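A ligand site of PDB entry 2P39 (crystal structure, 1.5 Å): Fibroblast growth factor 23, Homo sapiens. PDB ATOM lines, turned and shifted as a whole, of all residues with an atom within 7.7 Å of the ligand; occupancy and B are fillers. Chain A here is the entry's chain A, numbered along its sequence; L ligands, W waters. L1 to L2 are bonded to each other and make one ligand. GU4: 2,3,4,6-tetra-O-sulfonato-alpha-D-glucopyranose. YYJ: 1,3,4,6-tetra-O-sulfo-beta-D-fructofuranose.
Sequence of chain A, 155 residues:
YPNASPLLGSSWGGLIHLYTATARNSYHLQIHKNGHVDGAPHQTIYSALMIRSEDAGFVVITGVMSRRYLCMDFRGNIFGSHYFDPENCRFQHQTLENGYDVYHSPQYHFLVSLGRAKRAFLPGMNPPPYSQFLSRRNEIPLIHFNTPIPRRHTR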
ATOM      1  N   THR A  20     -21.183  22.172  27.043  1.00  0.00           N
ATOM      2  CA  THR A  20     -20.584  21.094  26.252  1.00  0.00           C
ATOM      3  C   THR A  20     -21.412  19.813  26.453  1.00  0.00           C
ATOM      4  O   THR A  20     -20.971  18.853  27.101  1.00  0.00           O
ATOM      5  CB  THR A  20     -19.104  20.869  26.639  1.00  0.00           C
ATOM      6  OG1 THR A  20     -18.986  20.749  28.060  1.00  0.00           O
ATOM      7  CG2 THR A  20     -18.266  22.039  26.172  1.00  0.00           C
ATOM      8  N   THR A  22     -22.214  17.244  24.613  1.00  0.00           N
ATOM      9  CA  THR A  22     -21.769  15.936  24.136  1.00  0.00           C
ATOM     10  C   THR A  22     -20.423  15.460  24.674  1.00  0.00           C
ATOM     11  O   THR A  22     -19.971  14.367  24.332  1.00  0.00           O
ATOM     12  CB  THR A  22     -21.732  15.900  22.584  1.00  0.00           C
ATOM     13  OG1 THR A  22     -20.866  16.934  22.096  1.00  0.00           O
ATOM     14  CG2 THR A  22     -23.125  16.097  22.009  1.00  0.00           C
ATOM     15  N   ALA A  23     -19.789  16.271  25.511  1.00  0.00           N
ATOM     16  CA  ALA A  23     -18.511  15.890  26.099  1.00  0.00           C
ATOM     17  C   ALA A  23     -18.735  14.817  27.169  1.00  0.00           C
ATOM     18  O   ALA A  23     -19.841  14.689  27.689  1.00  0.00           O
ATOM     19  CB  ALA A  23     -17.830  17.111  26.707  1.00  0.00           C
ATOM     20  N   ARG A  24     -17.683  14.056  27.492  1.00  0.00           N
ATOM     21  CA  ARG A  24     -17.797  13.034  28.524  1.00  0.00           C
ATOM     22  C   ARG A  24     -18.149  13.741  29.830  1.00  0.00           C
ATOM     23  O   ARG A  24     -18.974  13.261  30.611  1.00  0.00           O
ATOM     24  CB  ARG A  24     -16.467  12.283  28.688  1.00  0.00           C
ATOM     25  CG  ARG A  24     -16.011  11.536  27.444  1.00  0.00           C
ATOM     26  CD  ARG A  24     -16.791  10.258  27.214  1.00  0.00           C
ATOM     27  NE  ARG A  24     -16.389   9.606  25.961  1.00  0.00           N
ATOM     28  CZ  ARG A  24     -15.177   9.128  25.705  1.00  0.00           C
ATOM     29  NH1 ARG A  24     -14.218   9.219  26.617  1.00  0.00           N
ATOM     30  NH2 ARG A  24     -14.917   8.569  24.531  1.00  0.00           N
ATOM     31  N   ASN A  25     -17.511  14.883  30.068  1.00  0.00           N
ATOM     32  CA  ASN A  25     -17.760  15.702  31.251  1.00  0.00           C
ATOM     33  C   ASN A  25     -18.303  17.022  30.692  1.00  0.00           C
ATOM     34  O   ASN A  25     -17.571  17.758  30.038  1.00  0.00           O
ATOM     35  CB  ASN A  25     -16.474  15.928  32.035  1.00  0.00           C
ATOM     36  CG  ASN A  25     -15.909  14.640  32.607  1.00  0.00           C
ATOM     37  OD1 ASN A  25     -16.494  14.038  33.503  1.00  0.00           O
ATOM     38  ND2 ASN A  25     -14.765  14.210  32.084  1.00  0.00           N
ATOM     39  N   SER A  26     -19.580  17.285  30.942  1.00  0.00           N
ATOM     40  CA  SER A  26     -20.226  18.492  30.426  1.00  0.00           C
ATOM     41  C   SER A  26     -20.205  19.671  31.388  1.00  0.00           C
ATOM     42  O   SER A  26     -20.448  19.534  32.583  1.00  0.00           O
ATOM     43  CB  SER A  26     -21.679  18.169  30.067  1.00  0.00           C
ATOM     44  OG  SER A  26     -21.746  17.102  29.130  1.00  0.00           O
ATOM     45  N   TYR A  27     -19.910  20.848  30.839  1.00  0.00           N
ATOM     46  CA  TYR A  27     -19.851  22.070  31.647  1.00  0.00           C
ATOM     47  C   TYR A  27     -20.308  23.295  30.876  1.00  0.00           C
ATOM     48  O   TYR A  27     -20.423  23.267  29.649  1.00  0.00           O
ATOM     49  CB  TYR A  27     -18.424  22.361  32.129  1.00  0.00           C
ATOM     50  CG  TYR A  27     -17.707  21.219  32.813  1.00  0.00           C
ATOM     51  CD1 TYR A  27     -16.732  20.479  32.136  1.00  0.00           C
ATOM     52  CD2 TYR A  27     -17.960  20.917  34.145  1.00  0.00           C
ATOM     53  CE1 TYR A  27     -16.028  19.472  32.781  1.00  0.00           C
ATOM     54  CE2 TYR A  27     -17.252  19.905  34.802  1.00  0.00           C
ATOM     55  CZ  TYR A  27     -16.292  19.192  34.117  1.00  0.00           C
ATOM     56  OH  TYR A  27     -15.564  18.221  34.784  1.00  0.00           O
ATOM     57  N   SER A 113     -12.787  25.336  23.172  1.00  0.00           N
ATOM     58  CA  SER A 113     -13.052  24.173  24.023  1.00  0.00           C
ATOM     59  C   SER A 113     -12.485  24.479  25.398  1.00  0.00           C
ATOM     60  O   SER A 113     -11.597  25.335  25.544  1.00  0.00           O
ATOM     61  CB  SER A 113     -12.452  22.896  23.440  1.00  0.00           C
ATOM     62  OG  SER A 113     -11.043  22.915  23.422  1.00  0.00           O
ATOM     63  N   LEU A 114     -12.989  23.788  26.408  1.00  0.00           N
ATOM     64  CA  LEU A 114     -12.592  24.054  27.796  1.00  0.00           C
ATOM     65  C   LEU A 114     -11.329  23.411  28.320  1.00  0.00           C
ATOM     66  O   LEU A 114     -10.733  23.906  29.293  1.00  0.00           O
ATOM     67  CB  LEU A 114     -13.752  23.690  28.724  1.00  0.00           C
ATOM     68  CG  LEU A 114     -15.141  24.184  28.300  1.00  0.00           C
ATOM     69  CD1 LEU A 114     -16.157  23.810  29.368  1.00  0.00           C
ATOM     70  CD2 LEU A 114     -15.117  25.692  28.087  1.00  0.00           C
ATOM     71  N   GLY A 115     -10.900  22.316  27.701  1.00  0.00           N
ATOM     72  CA  GLY A 115      -9.721  21.606  28.162  1.00  0.00           C
ATOM     73  C   GLY A 115      -8.408  21.890  27.464  1.00  0.00           C
ATOM     74  O   GLY A 115      -8.308  22.801  26.646  1.00  0.00           O
ATOM     75  N   ARG A 116      -7.397  21.081  27.774  1.00  0.00           N
ATOM     76  CA  ARG A 116      -6.074  21.248  27.186  1.00  0.00           C
ATOM     77  C   ARG A 116      -5.949  20.718  25.757  1.00  0.00           C
ATOM     78  O   ARG A 116      -5.093  21.172  25.005  1.00  0.00           O
ATOM     79  CB  ARG A 116      -5.020  20.561  28.072  1.00  0.00           C
ATOM     80  CG  ARG A 116      -5.246  19.067  28.235  1.00  0.00           C
ATOM     81  CD  ARG A 116      -4.150  18.418  29.060  1.00  0.00           C
ATOM     82  NE  ARG A 116      -4.446  17.009  29.300  1.00  0.00           N
ATOM     83  CZ  ARG A 116      -3.590  16.137  29.823  1.00  0.00           C
ATOM     84  NH1 ARG A 116      -2.372  16.518  30.175  1.00  0.00           N
ATOM     85  NH2 ARG A 116      -3.958  14.874  29.999  1.00  0.00           N
ATOM     86  N   ALA A 117      -6.808  19.773  25.387  1.00  0.00           N
ATOM     87  CA  ALA A 117      -6.761  19.220  24.044  1.00  0.00           C
ATOM     88  C   ALA A 117      -7.378  20.214  23.069  1.00  0.00           C
ATOM     89  O   ALA A 117      -8.584  20.427  23.065  1.00  0.00           O
ATOM     90  CB  ALA A 117      -7.517  17.893  24.001  1.00  0.00           C
ATOM     91  N   LYS A 118      -6.525  20.824  22.243  1.00  0.00           N
ATOM     92  CA  LYS A 118      -6.993  21.806  21.273  1.00  0.00           C
ATOM     93  C   LYS A 118      -7.009  21.206  19.877  1.00  0.00           C
ATOM     94  O   LYS A 118      -6.041  20.579  19.443  1.00  0.00           O
ATOM     95  CB  LYS A 118      -6.088  23.047  21.301  1.00  0.00           C
ATOM     96  CG  LYS A 118      -6.039  23.737  22.658  1.00  0.00           C
ATOM     97  CD  LYS A 118      -7.449  24.048  23.163  1.00  0.00           C
ATOM     98  CE  LYS A 118      -7.425  24.796  24.487  1.00  0.00           C
ATOM     99  NZ  LYS A 118      -8.794  24.983  25.019  1.00  0.00           N
ATOM    100  N   ARG A 119      -8.124  21.394  19.174  1.00  0.00           N
ATOM    101  CA  ARG A 119      -8.292  20.846  17.845  1.00  0.00           C
ATOM    102  C   ARG A 119      -8.724  21.901  16.844  1.00  0.00           C
ATOM    103  O   ARG A 119      -9.562  22.751  17.142  1.00  0.00           O
ATOM    104  CB  ARG A 119      -9.351  19.740  17.868  1.00  0.00           C
ATOM    105  CG  ARG A 119      -9.384  18.870  16.627  1.00  0.00           C
ATOM    106  CD  ARG A 119      -8.041  18.183  16.440  1.00  0.00           C
ATOM    107  NE  ARG A 119      -7.632  17.497  17.667  1.00  0.00           N
ATOM    108  CZ  ARG A 119      -6.378  17.188  17.966  1.00  0.00           C
ATOM    109  NH1 ARG A 119      -5.393  17.506  17.146  1.00  0.00           N
ATOM    110  NH2 ARG A 119      -6.112  16.558  19.109  1.00  0.00           N
ATOM    111  N   PRO A 127     -15.651  17.692  14.063  1.00  0.00           N
ATOM    112  CA  PRO A 127     -15.008  18.192  15.283  1.00  0.00           C
ATOM    113  C   PRO A 127     -15.294  17.202  16.420  1.00  0.00           C
ATOM    114  O   PRO A 127     -16.300  16.480  16.384  1.00  0.00           O
ATOM    115  CB  PRO A 127     -15.685  19.540  15.500  1.00  0.00           C
ATOM    116  CG  PRO A 127     -17.062  19.322  14.960  1.00  0.00           C
ATOM    117  CD  PRO A 127     -16.781  18.555  13.677  1.00  0.00           C
ATOM    118  N   PRO A 128     -14.409  17.129  17.426  1.00  0.00           N
ATOM    119  CA  PRO A 128     -14.635  16.194  18.534  1.00  0.00           C
ATOM    120  C   PRO A 128     -15.817  16.612  19.411  1.00  0.00           C
ATOM    121  O   PRO A 128     -16.152  17.795  19.491  1.00  0.00           O
ATOM    122  CB  PRO A 128     -13.299  16.227  19.284  1.00  0.00           C
ATOM    123  CG  PRO A 128     -12.848  17.638  19.075  1.00  0.00           C
ATOM    124  CD  PRO A 128     -13.157  17.889  17.613  1.00  0.00           C
ATOM    125  N   PRO A 129     -16.454  15.645  20.074  1.00  0.00           N
ATOM    126  CA  PRO A 129     -17.598  15.954  20.938  1.00  0.00           C
ATOM    127  C   PRO A 129     -17.346  17.030  21.985  1.00  0.00           C
ATOM    128  O   PRO A 129     -18.233  17.836  22.282  1.00  0.00           O
ATOM    129  CB  PRO A 129     -17.929  14.604  21.565  1.00  0.00           C
ATOM    130  CG  PRO A 129     -17.564  13.631  20.485  1.00  0.00           C
ATOM    131  CD  PRO A 129     -16.243  14.188  19.983  1.00  0.00           C
ATOM    132  N   TYR A 130     -16.146  17.076  22.546  1.00  0.00           N
ATOM    133  CA  TYR A 130     -15.856  18.056  23.585  1.00  0.00           C
ATOM    134  C   TYR A 130     -15.831  19.511  23.092  1.00  0.00           C
ATOM    135  O   TYR A 130     -15.775  20.436  23.906  1.00  0.00           O
ATOM    136  CB  TYR A 130     -14.537  17.717  24.302  1.00  0.00           C
ATOM    137  CG  TYR A 130     -13.274  17.837  23.478  1.00  0.00           C
ATOM    138  CD1 TYR A 130     -12.791  19.080  23.070  1.00  0.00           C
ATOM    139  CD2 TYR A 130     -12.539  16.699  23.126  1.00  0.00           C
ATOM    140  CE1 TYR A 130     -11.609  19.186  22.329  1.00  0.00           C
ATOM    141  CE2 TYR A 130     -11.367  16.803  22.387  1.00  0.00           C
ATOM    142  CZ  TYR A 130     -10.910  18.048  21.996  1.00  0.00           C
ATOM    143  OH  TYR A 130      -9.745  18.156  21.269  1.00  0.00           O
ATOM    144  N   SER A 131     -15.885  19.703  21.780  1.00  0.00           N
ATOM    145  CA  SER A 131     -15.862  21.058  21.210  1.00  0.00           C
ATOM    146  C   SER A 131     -17.251  21.513  20.771  1.00  0.00           C
ATOM    147  O   SER A 131     -17.411  22.618  20.249  1.00  0.00           O
ATOM    148  CB  SER A 131     -14.917  21.115  20.003  1.00  0.00           C
ATOM    149  OG  SER A 131     -15.445  20.389  18.898  1.00  0.00           O
ATOM    150  N   GLN A 132     -18.250  20.666  20.985  1.00  0.00           N
ATOM    151  CA  GLN A 132     -19.617  20.999  20.588  1.00  0.00           C
ATOM    152  C   GLN A 132     -20.410  21.659  21.713  1.00  0.00           C
ATOM    153  O   GLN A 132     -20.338  21.247  22.865  1.00  0.00           O
ATOM    154  CB  GLN A 132     -20.313  19.727  20.098  1.00  0.00           C
ATOM    155  CG  GLN A 132     -19.659  19.157  18.838  1.00  0.00           C
ATOM    156  CD  GLN A 132     -20.349  17.923  18.306  1.00  0.00           C
ATOM    157  OE1 GLN A 132     -20.091  17.502  17.169  1.00  0.00           O
ATOM    158  NE2 GLN A 132     -21.221  17.331  19.106  1.00  0.00           N
HETATM  159  C1  GU4 L   1     -10.803  12.222  28.258  1.00  0.00           C
HETATM  160  O5  GU4 L   1     -10.240  13.082  29.269  1.00  0.00           O
HETATM  161  C5  GU4 L   1     -11.087  13.238  30.408  1.00  0.00           C
HETATM  162  C6  GU4 L   1     -10.395  14.320  31.204  1.00  0.00           C
HETATM  163  O6  GU4 L   1      -9.109  13.919  31.664  1.00  0.00           O
HETATM  164  S6  GU4 L   1      -8.304  14.764  32.524  1.00  0.00           S
HETATM  165  O22 GU4 L   1      -8.879  14.878  33.847  1.00  0.00           O
HETATM  166  O23 GU4 L   1      -8.133  16.088  31.991  1.00  0.00           O
HETATM  167  O21 GU4 L   1      -7.003  14.142  32.587  1.00  0.00           O
HETATM  168  C4  GU4 L   1     -11.358  11.851  31.051  1.00  0.00           C
HETATM  169  O4  GU4 L   1     -12.463  12.003  31.969  1.00  0.00           O
HETATM  170  S4  GU4 L   1     -12.284  11.597  33.365  1.00  0.00           S
HETATM  171  O25 GU4 L   1     -13.415  12.085  34.072  1.00  0.00           O
HETATM  172  O26 GU4 L   1     -11.127  12.245  33.853  1.00  0.00           O
HETATM  173  O24 GU4 L   1     -12.231  10.155  33.540  1.00  0.00           O
HETATM  174  C3  GU4 L   1     -11.914  10.860  29.987  1.00  0.00           C
HETATM  175  O3  GU4 L   1     -12.129   9.540  30.552  1.00  0.00           O
HETATM  176  S3  GU4 L   1     -13.431   8.835  30.543  1.00  0.00           S
HETATM  177  O28 GU4 L   1     -13.819   8.337  29.229  1.00  0.00           O
HETATM  178  O29 GU4 L   1     -14.499   9.724  30.966  1.00  0.00           O
HETATM  179  O27 GU4 L   1     -13.334   7.704  31.476  1.00  0.00           O
HETATM  180  C2  GU4 L   1     -10.927  10.797  28.817  1.00  0.00           C
HETATM  181  O2  GU4 L   1     -11.292   9.866  27.749  1.00  0.00           O
HETATM  182  S2  GU4 L   1     -10.284   9.022  27.047  1.00  0.00           S
HETATM  183  O11 GU4 L   1     -11.014   8.141  26.141  1.00  0.00           O
HETATM  184  O12 GU4 L   1      -9.501   8.235  28.010  1.00  0.00           O
HETATM  185  O10 GU4 L   1      -9.343   9.841  26.305  1.00  0.00           O
HETATM  186  C1  YYJ L   2     -13.589  13.215  25.975  1.00  0.00           C
HETATM  187  C2  YYJ L   2     -12.269  13.583  26.660  1.00  0.00           C
HETATM  188  C3  YYJ L   2     -12.231  15.089  26.953  1.00  0.00           C
HETATM  189  C4  YYJ L   2     -10.768  15.475  26.760  1.00  0.00           C
HETATM  190  C5  YYJ L   2     -10.454  14.677  25.517  1.00  0.00           C
HETATM  191  C6  YYJ L   2      -8.978  14.340  25.360  1.00  0.00           C
HETATM  192  O1  YYJ L   2     -13.742  13.844  24.671  1.00  0.00           O
HETATM  193 O1S1 YYJ L   2     -16.086  14.189  24.776  1.00  0.00           O
HETATM  194 O1S3 YYJ L   2     -13.859  17.243  27.990  1.00  0.00           O
HETATM  195 O1S4 YYJ L   2      -9.786  17.555  28.791  1.00  0.00           O
HETATM  196 O1S6 YYJ L   2      -7.829  12.415  22.345  1.00  0.00           O
HETATM  197  O2  YYJ L   2     -12.084  12.717  27.809  1.00  0.00           O
HETATM  198 O2S1 YYJ L   2     -15.201  12.261  23.723  1.00  0.00           O
HETATM  199 O2S3 YYJ L   2     -13.869  16.158  30.069  1.00  0.00           O
HETATM  200 O2S4 YYJ L   2      -9.258  18.838  26.849  1.00  0.00           O
HETATM  201 O2S6 YYJ L   2      -6.497  12.723  24.233  1.00  0.00           O
HETATM  202  O3  YYJ L   2     -12.503  15.367  28.332  1.00  0.00           O
HETATM  203 O3S1 YYJ L   2     -14.985  14.448  22.725  1.00  0.00           O
HETATM  204 O3S3 YYJ L   2     -14.864  15.076  28.279  1.00  0.00           O
HETATM  205 O3S4 YYJ L   2      -8.270  16.724  27.252  1.00  0.00           O
HETATM  206 O3S6 YYJ L   2      -7.241  14.578  22.923  1.00  0.00           O
HETATM  207  O4  YYJ L   2     -10.625  16.904  26.613  1.00  0.00           O
HETATM  208  O5  YYJ L   2     -11.187  13.427  25.693  1.00  0.00           O
HETATM  209  O6  YYJ L   2      -8.786  13.390  24.263  1.00  0.00           O
HETATM  210  S1  YYJ L   2     -15.005  13.675  23.956  1.00  0.00           S
HETATM  211  S3  YYJ L   2     -13.783  15.967  28.647  1.00  0.00           S
HETATM  212  S4  YYJ L   2      -9.485  17.506  27.365  1.00  0.00           S
HETATM  213  S6  YYJ L   2      -7.582  13.285  23.458  1.00  0.00           S
HETATM  214  O   HOH W   1     -13.850  19.883  28.362  1.00  0.00           O
HETATM  215  O   HOH W   2     -10.898  20.846  25.323  1.00  0.00           O
HETATM  216  O   HOH W   3      -8.794   7.562  30.677  1.00  0.00           O
HETATM  217  O   HOH W   4     -18.233  12.156  24.247  1.00  0.00           O
HETATM  218  O   HOH W   5      -7.707  19.559  30.243  1.00  0.00           O
HETATM  219  O   HOH W   6      -8.218  16.029  20.785  1.00  0.00           O
HETATM  220  O   HOH W   7     -14.536  10.895  21.369  1.00  0.00           O
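N of Pro 129 lies close to O3S1 of YYJ L2 (3.3 Å). Thr 22 touches the ligand. Ala 23 touches the ligand. Gly 115 touches the ligand. Hydrophobic or aromatic side chains that line the ligand: Ala 23, Ala 117, Pro 129 and Tyr 130. Of the 20 residues printed, 9 come within 4 Å of the ligand.
The backbone carbonyl oxygen (O) of Pro 129 lies within hydrogen-bond range of the side-chain hydroxyl (OG1) of Thr 22, at 2.8 Å. O of Ala 23 is in hydrogen-bond range of OG of Ser 26, 3.4 Å away. O of Gly 115 lies within hydrogen-bond range of NZ of Lys 118, at 2.8 Å. The side-chain hydroxyl (OG1) of Thr 22 sits at hydrogen-bond distance from the side-chain amide nitrogen (NE2) of Gln 132 (3.0 Å). The backbone carbonyl oxygen of Ala 117 lies within hydrogen-bond range of the side-chain hydroxyl of Tyr 130, 3.1 Å away.
Water W6 lies within hydrogen-bond range of OH of Tyr 130 (2.7 Å), NH2 of Arg 119 (2.7 Å) and O3S6 of YYJ L2 (2.8 Å). Water W4 bridges the backbone carbonyl oxygen of Thr 22 (2.8 Å) and an oxygen (O1S1) of YYJ L2 (3.0 Å). Water W2 lies within hydrogen-bond range of the backbone NH of Gly 115 (2.8 Å), the side-chain hydroxyl of Ser 113 (2.8 Å), an oxygen (O2S4) of YYJ L2 (3.0 Å) and the backbone carbonyl oxygen of Ala 117 (3.3 Å). Water W5 bridges the backbone NH of Arg 116 and an oxygen (O1S4) of YYJ L2.
The backbone NH (N) of Arg 116 lies within hydrogen-bond range of an oxygen (O2S4) of YYJ L2. O28 of GU4 L1 lies within salt-bridge range of NH1 of Arg 24. The side-chain amide nitrogen (ND2) of Asn 25 is in hydrogen-bond range of an oxygen (O2S3) of YYJ L2, 2.9 Å away. An oxygen (O3S3) of YYJ L2 lies within hydrogen-bond range of the backbone NH of Arg 24 (3.1 Å). The backbone NH (N) of Tyr 130 is in hydrogen-bond range of an oxygen (O3S1) of YYJ L2 (2.9 Å). The backbone NH (N) of Ala 117 sits at hydrogen-bond distance from an oxygen (O2S4) of YYJ L2. The backbone NH (N) of Asn 25 lies within hydrogen-bond range of an oxygen (O3S3) of YYJ L2 (3.2 Å).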
